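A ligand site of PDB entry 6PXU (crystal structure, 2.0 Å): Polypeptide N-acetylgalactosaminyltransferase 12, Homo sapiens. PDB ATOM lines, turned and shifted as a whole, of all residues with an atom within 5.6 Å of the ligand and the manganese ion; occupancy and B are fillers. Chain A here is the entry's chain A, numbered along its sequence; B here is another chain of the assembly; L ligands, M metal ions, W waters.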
ATOM      1  N   ILE A 104      18.818  -2.560  22.588  1.00  0.00           N
ATOM      2  CA  ILE A 104      18.659  -1.130  22.875  1.00  0.00           C
ATOM      3  C   ILE A 104      18.141  -0.466  21.603  1.00  0.00           C
ATOM      4  O   ILE A 104      18.934  -0.093  20.724  1.00  0.00           O
ATOM      5  CB  ILE A 104      19.971  -0.480  23.334  1.00  0.00           C
ATOM      6  CG1 ILE A 104      20.517  -1.184  24.581  1.00  0.00           C
ATOM      7  CG2 ILE A 104      19.752   1.031  23.568  1.00  0.00           C
ATOM      8  CD1 ILE A 104      21.910  -0.723  25.003  1.00  0.00           C
ATOM      9  N   ALA A 105      16.840  -0.282  21.501  1.00  0.00           N
ATOM     10  CA  ALA A 105      16.282   0.515  20.413  1.00  0.00           C
ATOM     11  C   ALA A 105      16.419   2.005  20.759  1.00  0.00           C
ATOM     12  O   ALA A 105      16.310   2.397  21.925  1.00  0.00           O
ATOM     13  CB  ALA A 105      14.828   0.124  20.174  1.00  0.00           C
ATOM     14  N   PHE A 106      16.732   2.822  19.762  1.00  0.00           N
ATOM     15  CA  PHE A 106      16.926   4.235  20.006  1.00  0.00           C
ATOM     16  C   PHE A 106      16.352   5.049  18.873  1.00  0.00           C
ATOM     17  O   PHE A 106      16.370   4.635  17.698  1.00  0.00           O
ATOM     18  CB  PHE A 106      18.423   4.611  20.238  1.00  0.00           C
ATOM     19  CG  PHE A 106      19.319   4.450  19.033  1.00  0.00           C
ATOM     20  CD1 PHE A 106      19.480   5.492  18.133  1.00  0.00           C
ATOM     21  CD2 PHE A 106      20.040   3.291  18.833  1.00  0.00           C
ATOM     22  CE1 PHE A 106      20.307   5.375  17.035  1.00  0.00           C
ATOM     23  CE2 PHE A 106      20.903   3.170  17.746  1.00  0.00           C
ATOM     24  CZ  PHE A 106      21.036   4.212  16.847  1.00  0.00           C
ATOM     25  N   TYR A 107      15.783   6.202  19.236  1.00  0.00           N
ATOM     26  CA  TYR A 107      15.209   7.141  18.275  1.00  0.00           C
ATOM     27  C   TYR A 107      15.647   8.539  18.663  1.00  0.00           C
ATOM     28  O   TYR A 107      15.141   9.096  19.647  1.00  0.00           O
ATOM     29  CB  TYR A 107      13.683   7.036  18.238  1.00  0.00           C
ATOM     30  CG  TYR A 107      13.080   8.118  17.369  1.00  0.00           C
ATOM     31  CD1 TYR A 107      13.290   8.127  16.006  1.00  0.00           C
ATOM     32  CD2 TYR A 107      12.335   9.146  17.934  1.00  0.00           C
ATOM     33  CE1 TYR A 107      12.776   9.127  15.225  1.00  0.00           C
ATOM     34  CE2 TYR A 107      11.800  10.149  17.159  1.00  0.00           C
ATOM     35  CZ  TYR A 107      12.031  10.138  15.801  1.00  0.00           C
ATOM     36  OH  TYR A 107      11.517  11.113  15.001  1.00  0.00           O
ATOM     37  N   GLU A 109      18.163   9.791  20.096  1.00  0.00           N
ATOM     38  CA  GLU A 109      18.824   9.999  21.376  1.00  0.00           C
ATOM     39  C   GLU A 109      20.081  10.854  21.184  1.00  0.00           C
ATOM     40  O   GLU A 109      20.716  10.841  20.129  1.00  0.00           O
ATOM     41  CB  GLU A 109      19.194   8.638  21.999  1.00  0.00           C
ATOM     42  CG  GLU A 109      19.727   8.696  23.438  1.00  0.00           C
ATOM     43  CD  GLU A 109      18.711   9.283  24.423  1.00  0.00           C
ATOM     44  OE1 GLU A 109      17.487   9.088  24.214  1.00  0.00           O
ATOM     45  OE2 GLU A 109      19.128   9.953  25.400  1.00  0.00           O
ATOM     46  N   VAL A 136      19.411  -0.855  17.903  1.00  0.00           N
ATOM     47  CA  VAL A 136      18.464  -0.756  16.796  1.00  0.00           C
ATOM     48  C   VAL A 136      18.123   0.709  16.604  1.00  0.00           C
ATOM     49  O   VAL A 136      17.420   1.313  17.414  1.00  0.00           O
ATOM     50  CB  VAL A 136      17.186  -1.576  17.042  1.00  0.00           C
ATOM     51  CG1 VAL A 136      16.344  -1.581  15.772  1.00  0.00           C
ATOM     52  CG2 VAL A 136      17.553  -2.989  17.495  1.00  0.00           C
ATOM     53  N   ASP A 138      15.913   3.242  15.207  1.00  0.00           N
ATOM     54  CA  ASP A 138      14.548   3.323  14.698  1.00  0.00           C
ATOM     55  C   ASP A 138      14.380   4.531  13.777  1.00  0.00           C
ATOM     56  O   ASP A 138      13.538   5.401  13.981  1.00  0.00           O
ATOM     57  CB  ASP A 138      13.541   3.369  15.862  1.00  0.00           C
ATOM     58  CG  ASP A 138      12.101   3.339  15.368  1.00  0.00           C
ATOM     59  OD1 ASP A 138      11.893   2.911  14.203  1.00  0.00           O
ATOM     60  OD2 ASP A 138      11.190   3.726  16.153  1.00  0.00           O
ATOM     61  N   ARG A 167      10.448   4.443   9.971  1.00  0.00           N
ATOM     62  CA  ARG A 167      10.079   4.618  11.366  1.00  0.00           C
ATOM     63  C   ARG A 167       9.239   3.424  11.821  1.00  0.00           C
ATOM     64  O   ARG A 167       8.192   3.115  11.228  1.00  0.00           O
ATOM     65  CB  ARG A 167       9.325   5.940  11.526  1.00  0.00           C
ATOM     66  CG  ARG A 167       8.961   6.248  12.960  1.00  0.00           C
ATOM     67  CD  ARG A 167      10.191   6.549  13.802  1.00  0.00           C
ATOM     68  NE  ARG A 167       9.838   6.650  15.212  1.00  0.00           N
ATOM     69  CZ  ARG A 167       9.282   7.727  15.751  1.00  0.00           C
ATOM     70  NH1 ARG A 167       9.029   8.793  15.001  1.00  0.00           N
ATOM     71  NH2 ARG A 167       8.978   7.739  17.042  1.00  0.00           N
ATOM     72  N   GLU A 168       9.702   2.730  12.850  1.00  0.00           N
ATOM     73  CA  GLU A 168       9.003   1.539  13.319  1.00  0.00           C
ATOM     74  C   GLU A 168       8.235   1.757  14.603  1.00  0.00           C
ATOM     75  O   GLU A 168       7.214   1.104  14.814  1.00  0.00           O
ATOM     76  CB  GLU A 168      10.003   0.380  13.540  1.00  0.00           C
ATOM     77  CG  GLU A 168      10.685  -0.114  12.260  1.00  0.00           C
ATOM     78  CD  GLU A 168       9.732  -0.830  11.317  1.00  0.00           C
ATOM     79  OE1 GLU A 168       8.580  -1.125  11.698  1.00  0.00           O
ATOM     80  OE2 GLU A 168      10.136  -1.085  10.161  1.00  0.00           O
ATOM     81  N   GLY A 169       8.687   2.654  15.466  1.00  0.00           N
ATOM     82  CA  GLY A 169       8.172   2.700  16.820  1.00  0.00           C
ATOM     83  C   GLY A 169       8.914   1.710  17.695  1.00  0.00           C
ATOM     84  O   GLY A 169       9.554   0.771  17.216  1.00  0.00           O
ATOM     85  N   LEU A 170       8.833   1.930  19.015  1.00  0.00           N
ATOM     86  CA  LEU A 170       9.663   1.157  19.924  1.00  0.00           C
ATOM     87  C   LEU A 170       9.306  -0.325  19.913  1.00  0.00           C
ATOM     88  O   LEU A 170      10.191  -1.176  20.043  1.00  0.00           O
ATOM     89  CB  LEU A 170       9.612   1.730  21.342  1.00  0.00           C
ATOM     90  CG  LEU A 170       8.427   1.555  22.271  1.00  0.00           C
ATOM     91  CD1 LEU A 170       8.551   0.285  23.082  1.00  0.00           C
ATOM     92  CD2 LEU A 170       8.335   2.773  23.180  1.00  0.00           C
ATOM     93  N   ALA A 173      10.763  -1.800  16.571  1.00  0.00           N
ATOM     94  CA  ALA A 173      12.213  -1.702  16.639  1.00  0.00           C
ATOM     95  C   ALA A 173      12.795  -2.735  17.603  1.00  0.00           C
ATOM     96  O   ALA A 173      13.822  -3.373  17.304  1.00  0.00           O
ATOM     97  CB  ALA A 173      12.636  -0.281  17.046  1.00  0.00           C
ATOM     98  N   ARG A 174      12.146  -2.894  18.763  1.00  0.00           N
ATOM     99  CA  ARG A 174      12.551  -3.949  19.683  1.00  0.00           C
ATOM    100  C   ARG A 174      12.440  -5.320  19.046  1.00  0.00           C
ATOM    101  O   ARG A 174      13.304  -6.170  19.235  1.00  0.00           O
ATOM    102  CB  ARG A 174      11.701  -3.920  20.941  1.00  0.00           C
ATOM    103  CG  ARG A 174      12.204  -2.932  21.903  1.00  0.00           C
ATOM    104  CD  ARG A 174      11.328  -2.766  23.096  1.00  0.00           C
ATOM    105  NE  ARG A 174      12.169  -2.068  24.036  1.00  0.00           N
ATOM    106  CZ  ARG A 174      11.776  -1.430  25.117  1.00  0.00           C
ATOM    107  NH1 ARG A 174      12.713  -0.838  25.855  1.00  0.00           N
ATOM    108  NH2 ARG A 174      10.487  -1.358  25.427  1.00  0.00           N
ATOM    109  N   LEU A 189      16.884  -2.722  27.325  1.00  0.00           N
ATOM    110  CA  LEU A 189      17.212  -1.471  28.006  1.00  0.00           C
ATOM    111  C   LEU A 189      16.840  -0.297  27.099  1.00  0.00           C
ATOM    112  O   LEU A 189      16.709  -0.443  25.884  1.00  0.00           O
ATOM    113  CB  LEU A 189      18.697  -1.415  28.371  1.00  0.00           C
ATOM    114  CG  LEU A 189      19.216  -2.549  29.258  1.00  0.00           C
ATOM    115  CD1 LEU A 189      20.702  -2.352  29.455  1.00  0.00           C
ATOM    116  CD2 LEU A 189      18.512  -2.576  30.620  1.00  0.00           C
ATOM    117  N   ASP A 190      16.630   0.879  27.715  1.00  0.00           N
ATOM    118  CA  ASP A 190      16.493   2.115  26.961  1.00  0.00           C
ATOM    119  C   ASP A 190      17.867   2.675  26.624  1.00  0.00           C
ATOM    120  O   ASP A 190      18.886   2.297  27.212  1.00  0.00           O
ATOM    121  CB  ASP A 190      15.689   3.154  27.765  1.00  0.00           C
ATOM    122  CG  ASP A 190      14.213   2.817  27.864  1.00  0.00           C
ATOM    123  OD1 ASP A 190      13.786   1.754  27.348  1.00  0.00           O
ATOM    124  OD2 ASP A 190      13.474   3.605  28.485  1.00  0.00           O
ATOM    125  N   CYS A 191      17.889   3.633  25.713  1.00  0.00           N
ATOM    126  CA  CYS A 191      19.154   4.198  25.263  1.00  0.00           C
ATOM    127  C   CYS A 191      19.652   5.318  26.172  1.00  0.00           C
ATOM    128  O   CYS A 191      20.531   6.086  25.761  1.00  0.00           O
ATOM    129  CB  CYS A 191      19.004   4.696  23.827  1.00  0.00           C
ATOM    130  SG  CYS A 191      17.700   5.939  23.696  1.00  0.00           S
ATOM    131  N   HIS A 192      19.118   5.433  27.396  1.00  0.00           N
ATOM    132  CA  HIS A 192      19.591   6.437  28.348  1.00  0.00           C
ATOM    133  C   HIS A 192      19.559   5.806  29.738  1.00  0.00           C
ATOM    134  O   HIS A 192      18.876   6.260  30.647  1.00  0.00           O
ATOM    135  CB  HIS A 192      18.727   7.704  28.283  1.00  0.00           C
ATOM    136  CG  HIS A 192      17.298   7.413  27.995  1.00  0.00           C
ATOM    137  ND1 HIS A 192      16.719   7.691  26.775  1.00  0.00           N
ATOM    138  CD2 HIS A 192      16.359   6.768  28.723  1.00  0.00           C
ATOM    139  CE1 HIS A 192      15.462   7.267  26.784  1.00  0.00           C
ATOM    140  NE2 HIS A 192      15.218   6.716  27.962  1.00  0.00           N
ATOM    141  N   VAL A 296       4.643   3.649  17.806  1.00  0.00           N
ATOM    142  CA  VAL A 296       5.454   4.717  18.417  1.00  0.00           C
ATOM    143  C   VAL A 296       5.797   4.467  19.892  1.00  0.00           C
ATOM    144  O   VAL A 296       6.950   4.166  20.207  1.00  0.00           O
ATOM    145  CB  VAL A 296       4.769   6.089  18.247  1.00  0.00           C
ATOM    146  CG1 VAL A 296       5.670   7.188  18.828  1.00  0.00           C
ATOM    147  CG2 VAL A 296       4.453   6.364  16.773  1.00  0.00           C
ATOM    148  N   TRP A 297       4.823   4.628  20.792  1.00  0.00           N
ATOM    149  CA  TRP A 297       5.102   4.680  22.238  1.00  0.00           C
ATOM    150  C   TRP A 297       3.816   4.483  23.030  1.00  0.00           C
ATOM    151  O   TRP A 297       2.735   4.892  22.583  1.00  0.00           O
ATOM    152  CB  TRP A 297       5.740   6.008  22.653  1.00  0.00           C
ATOM    153  CG  TRP A 297       6.019   6.140  24.148  1.00  0.00           C
ATOM    154  CD1 TRP A 297       7.192   5.854  24.776  1.00  0.00           C
ATOM    155  CD2 TRP A 297       5.125   6.642  25.162  1.00  0.00           C
ATOM    156  NE1 TRP A 297       7.069   6.104  26.127  1.00  0.00           N
ATOM    157  CE2 TRP A 297       5.819   6.592  26.392  1.00  0.00           C
ATOM    158  CE3 TRP A 297       3.798   7.113  25.150  1.00  0.00           C
ATOM    159  CZ2 TRP A 297       5.243   6.997  27.586  1.00  0.00           C
ATOM    160  CZ3 TRP A 297       3.229   7.522  26.350  1.00  0.00           C
ATOM    161  CH2 TRP A 297       3.944   7.453  27.550  1.00  0.00           C
ATOM    162  N   HIS A 325      17.830   5.230  35.018  1.00  0.00           N
ATOM    163  CA  HIS A 325      17.129   5.607  33.793  1.00  0.00           C
ATOM    164  C   HIS A 325      16.940   7.123  33.795  1.00  0.00           C
ATOM    165  O   HIS A 325      16.484   7.676  34.806  1.00  0.00           O
ATOM    166  CB  HIS A 325      15.786   4.861  33.736  1.00  0.00           C
ATOM    167  CG  HIS A 325      14.902   5.264  32.597  1.00  0.00           C
ATOM    168  ND1 HIS A 325      14.038   6.342  32.664  1.00  0.00           N
ATOM    169  CD2 HIS A 325      14.738   4.734  31.364  1.00  0.00           C
ATOM    170  CE1 HIS A 325      13.380   6.460  31.533  1.00  0.00           C
ATOM    171  NE2 HIS A 325      13.787   5.495  30.718  1.00  0.00           N
ATOM    172  N   VAL A 326      17.325   7.796  32.721  1.00  0.00           N
ATOM    173  CA  VAL A 326      17.158   9.244  32.675  1.00  0.00           C
ATOM    174  C   VAL A 326      15.719   9.582  32.269  1.00  0.00           C
ATOM    175  O   VAL A 326      15.427   9.750  31.085  1.00  0.00           O
ATOM    176  CB  VAL A 326      18.132   9.939  31.710  1.00  0.00           C
ATOM    177  CG1 VAL A 326      18.003  11.475  31.867  1.00  0.00           C
ATOM    178  CG2 VAL A 326      19.528   9.498  31.981  1.00  0.00           C
ATOM    179  N   PRO A 328      12.923  11.887  31.323  1.00  0.00           N
ATOM    180  CA  PRO A 328      13.021  13.232  30.741  1.00  0.00           C
ATOM    181  C   PRO A 328      12.123  14.252  31.431  1.00  0.00           C
ATOM    182  O   PRO A 328      11.184  13.922  32.147  1.00  0.00           O
ATOM    183  CB  PRO A 328      12.598  12.994  29.293  1.00  0.00           C
ATOM    184  CG  PRO A 328      11.663  11.844  29.363  1.00  0.00           C
ATOM    185  CD  PRO A 328      12.181  10.956  30.460  1.00  0.00           C
ATOM    186  N   PRO A 332      10.057  13.661  24.901  1.00  0.00           N
ATOM    187  CA  PRO A 332      11.020  14.257  23.951  1.00  0.00           C
ATOM    188  C   PRO A 332      10.570  14.243  22.499  1.00  0.00           C
ATOM    189  O   PRO A 332      11.223  14.885  21.656  1.00  0.00           O
ATOM    190  CB  PRO A 332      12.282  13.383  24.136  1.00  0.00           C
ATOM    191  CG  PRO A 332      11.981  12.429  25.249  1.00  0.00           C
ATOM    192  CD  PRO A 332      10.494  12.339  25.379  1.00  0.00           C
ATOM    193  N   TYR A 333       9.482  13.548  22.178  1.00  0.00           N
ATOM    194  CA  TYR A 333       8.944  13.467  20.830  1.00  0.00           C
ATOM    195  C   TYR A 333       7.438  13.282  20.998  1.00  0.00           C
ATOM    196  O   TYR A 333       6.960  12.973  22.102  1.00  0.00           O
ATOM    197  CB  TYR A 333       9.602  12.322  20.038  1.00  0.00           C
ATOM    198  CG  TYR A 333       9.557  11.025  20.817  1.00  0.00           C
ATOM    199  CD1 TYR A 333       8.393  10.228  20.818  1.00  0.00           C
ATOM    200  CD2 TYR A 333      10.624  10.625  21.622  1.00  0.00           C
ATOM    201  CE1 TYR A 333       8.308   9.065  21.567  1.00  0.00           C
ATOM    202  CE2 TYR A 333      10.547   9.442  22.377  1.00  0.00           C
ATOM    203  CZ  TYR A 333       9.388   8.675  22.332  1.00  0.00           C
ATOM    204  OH  TYR A 333       9.282   7.524  23.083  1.00  0.00           O
ATOM    205  N   ARG A 335       4.041  11.855  21.423  1.00  0.00           N
ATOM    206  CA  ARG A 335       3.449  10.590  21.846  1.00  0.00           C
ATOM    207  C   ARG A 335       1.935  10.730  21.707  1.00  0.00           C
ATOM    208  O   ARG A 335       1.226  11.117  22.626  1.00  0.00           O
ATOM    209  CB  ARG A 335       3.884  10.243  23.240  1.00  0.00           C
ATOM    210  CG  ARG A 335       5.359   9.834  23.320  1.00  0.00           C
ATOM    211  CD  ARG A 335       5.861  10.023  24.724  1.00  0.00           C
ATOM    212  NE  ARG A 335       7.220   9.571  24.926  1.00  0.00           N
ATOM    213  CZ  ARG A 335       7.853   9.620  26.091  1.00  0.00           C
ATOM    214  NH1 ARG A 335       9.096   9.185  26.198  1.00  0.00           N
ATOM    215  NH2 ARG A 335       7.223  10.106  27.156  1.00  0.00           N
ATOM    216  N   ILE B  13       3.987  10.446  29.583  1.00  0.00           N
ATOM    217  CA  ILE B  13       5.274  10.203  30.233  1.00  0.00           C
ATOM    218  C   ILE B  13       5.173   8.958  31.113  1.00  0.00           C
ATOM    219  O   ILE B  13       4.088   8.576  31.576  1.00  0.00           O
ATOM    220  CB  ILE B  13       5.762  11.394  31.104  1.00  0.00           C
ATOM    221  CG1 ILE B  13       4.655  11.878  32.047  1.00  0.00           C
ATOM    222  CG2 ILE B  13       6.327  12.521  30.255  1.00  0.00           C
ATOM    223  CD1 ILE B  13       5.035  13.105  32.853  1.00  0.00           C
ATOM    224  N   THR B  14       6.324   8.329  31.349  1.00  0.00           N
ATOM    225  CA  THR B  14       6.448   7.281  32.351  1.00  0.00           C
ATOM    226  C   THR B  14       6.818   7.906  33.698  1.00  0.00           C
ATOM    227  O   THR B  14       7.823   8.619  33.779  1.00  0.00           O
ATOM    228  CB  THR B  14       7.494   6.263  31.947  1.00  0.00           C
ATOM    229  OG1 THR B  14       7.011   5.509  30.830  1.00  0.00           O
ATOM    230  CG2 THR B  14       7.810   5.300  33.087  1.00  0.00           C
HETATM  231  N1  LIG L   1      12.102   4.542  20.961  1.00  0.00           N
HETATM  232  C1  LIG L   1      12.218   4.035  19.676  1.00  0.00           C
HETATM  233  N2  LIG L   1      11.311   4.399  18.715  1.00  0.00           N
HETATM  234  C2  LIG L   1      10.288   5.269  19.056  1.00  0.00           C
HETATM  235  C3  LIG L   1      10.179   5.771  20.352  1.00  0.00           C
HETATM  236  C4  LIG L   1      11.114   5.415  21.324  1.00  0.00           C
HETATM  237  O1  LIG L   1      13.128   3.243  19.403  1.00  0.00           O
HETATM  238  O2  LIG L   1       9.497   5.575  18.183  1.00  0.00           O
HETATM  239  C5  LIG L   1      13.110   4.057  21.915  1.00  0.00           C
HETATM  240  C6  LIG L   1      13.688   5.118  22.838  1.00  0.00           C
HETATM  241  O3  LIG L   1      14.911   5.578  22.304  1.00  0.00           O
HETATM  242  C7  LIG L   1      13.897   4.300  24.095  1.00  0.00           C
HETATM  243  C8  LIG L   1      12.737   3.308  24.054  1.00  0.00           C
HETATM  244  O4  LIG L   1      12.535   3.042  22.716  1.00  0.00           O
HETATM  245  O5  LIG L   1      15.169   3.635  24.014  1.00  0.00           O
HETATM  246  C9  LIG L   1      11.412   3.997  24.356  1.00  0.00           C
HETATM  247  O6  LIG L   1      11.650   4.674  25.517  1.00  0.00           O
HETATM  248  P1  LIG L   1      11.488   6.241  25.850  1.00  0.00           P
HETATM  249  O7  LIG L   1      11.392   7.307  24.818  1.00  0.00           O
HETATM  250  O8  LIG L   1      12.658   6.420  26.747  1.00  0.00           O
HETATM  251  O9  LIG L   1      10.143   6.203  26.723  1.00  0.00           O
HETATM  252  P2  LIG L   1      10.096   6.448  28.316  1.00  0.00           P
HETATM  253  O10 LIG L   1       8.720   6.082  28.729  1.00  0.00           O
HETATM  254  O11 LIG L   1      10.403   7.880  28.581  1.00  0.00           O
HETATM  255  O12 LIG L   1      11.065   5.578  29.033  1.00  0.00           O
HETATM  256 MN    MN M   1      13.243   5.867  28.639  1.00  0.00          MN
HETATM  257  O   HOH W   1      12.843   8.158  29.140  1.00  0.00           O
HETATM  258  O   HOH W   2      13.388   9.232  24.245  1.00  0.00           O
HETATM  259  O   HOH W   3       8.403   9.309  29.772  1.00  0.00           O
HETATM  260  O   HOH W   4      15.543   8.151  22.738  1.00  0.00           O
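The guanidinium group (NH2) of Arg 167 sits at hydrogen-bond distance from an oxygen (O2) of the ligand (2.5 Å). The side-chain carboxylate (OD2) of Asp 138 is in hydrogen-bond range of a nitrogen (N2) of the ligand (2.7 Å). O5 of the ligand lies within hydrogen-bond range of O of Ala 105 (2.7 Å). The side-chain hydroxyl of Tyr 333 lies within hydrogen-bond range of an oxygen (O7) of the ligand (2.7 Å). An oxygen (O10) of the ligand lies within hydrogen-bond range of the side-chain hydroxyl (OG1) of Thr 14 of chain B (2.8 Å). The guanidinium group (NH1) of Arg 335 is in salt-bridge range of an oxygen (O11) of the ligand, 3.0 Å away. The indole nitrogen of Trp 297 is in hydrogen-bond range of an oxygen (O10) of the ligand. The backbone NH of Cys 191 lies within hydrogen-bond range of an oxygen (O5) of the ligand, 3.2 Å away. The side-chain sulfur of Cys 191 sits at hydrogen-bond distance from an oxygen (O3) of the ligand (3.1 Å). O3 of the ligand is in hydrogen-bond range of N of Tyr 107.
A ring nitrogen (ND1) of His 192 lies within hydrogen-bond range of the side-chain sulfur of Cys 191. The backbone NH of Val 326 is in hydrogen-bond range of the backbone carbonyl oxygen of His 192. The guanidinium group (NH1) of Arg 174 lies within salt-bridge range of the side-chain carboxylate (OD1) of Asp 190 (3.2 Å). NE of Arg 167 is in salt-bridge range of OD2 of Asp 138, at 3.4 Å. The side-chain hydroxyl (OH) of Tyr 107 lies close to the guanidinium group (NH1) of Arg 167. The side-chain carboxylate of Asp 138 lies within hydrogen-bond range of the backbone NH of Glu 168, 2.6 Å away. O of Val 136 is in hydrogen-bond range of N of Phe 106, 2.9 Å away. O of Val 296 is in hydrogen-bond range of N of Leu 170 (3.2 Å).
CA of Phe 106 touches O3 of the ligand (3.3 Å). Gly 169 touches the ligand (CA to O2, 3.4 Å). Leu 170 touches the ligand. Val 296 touches the ligand. Hydrophobic or aromatic side chains within 4 Å of the ligand: Ala 105, Tyr 107, Leu 170, His 192, Trp 297, His 325 and Tyr 333. Of the 27 residues printed, 16 come within 4 Å of the ligand. The nearest printed residue that does not touch the ligand is Pro 328 (4.02 Å).
Three residues have an atom within 4 Å of the manganese ion: Asp 190, His 192 and His 325. The nearest printed residue that does not touch the manganese ion is Val 326 (5.1 Å).
The manganese ion is bound by O8 of the ligand, NE2 of His 325, O12 of the ligand, NE2 of His 192, OD2 of Asp 190 and water W1.
Water W4 lies within hydrogen-bond range of OE1 of Glu 109, O3 of the ligand, SG of Cys 191 and O of Tyr 107. Water W3 lies within hydrogen-bond range of O11 of the ligand (2.7 Å), N of Thr 14 of chain B (2.8 Å) and NH2 of Arg 335 (3.0 Å).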
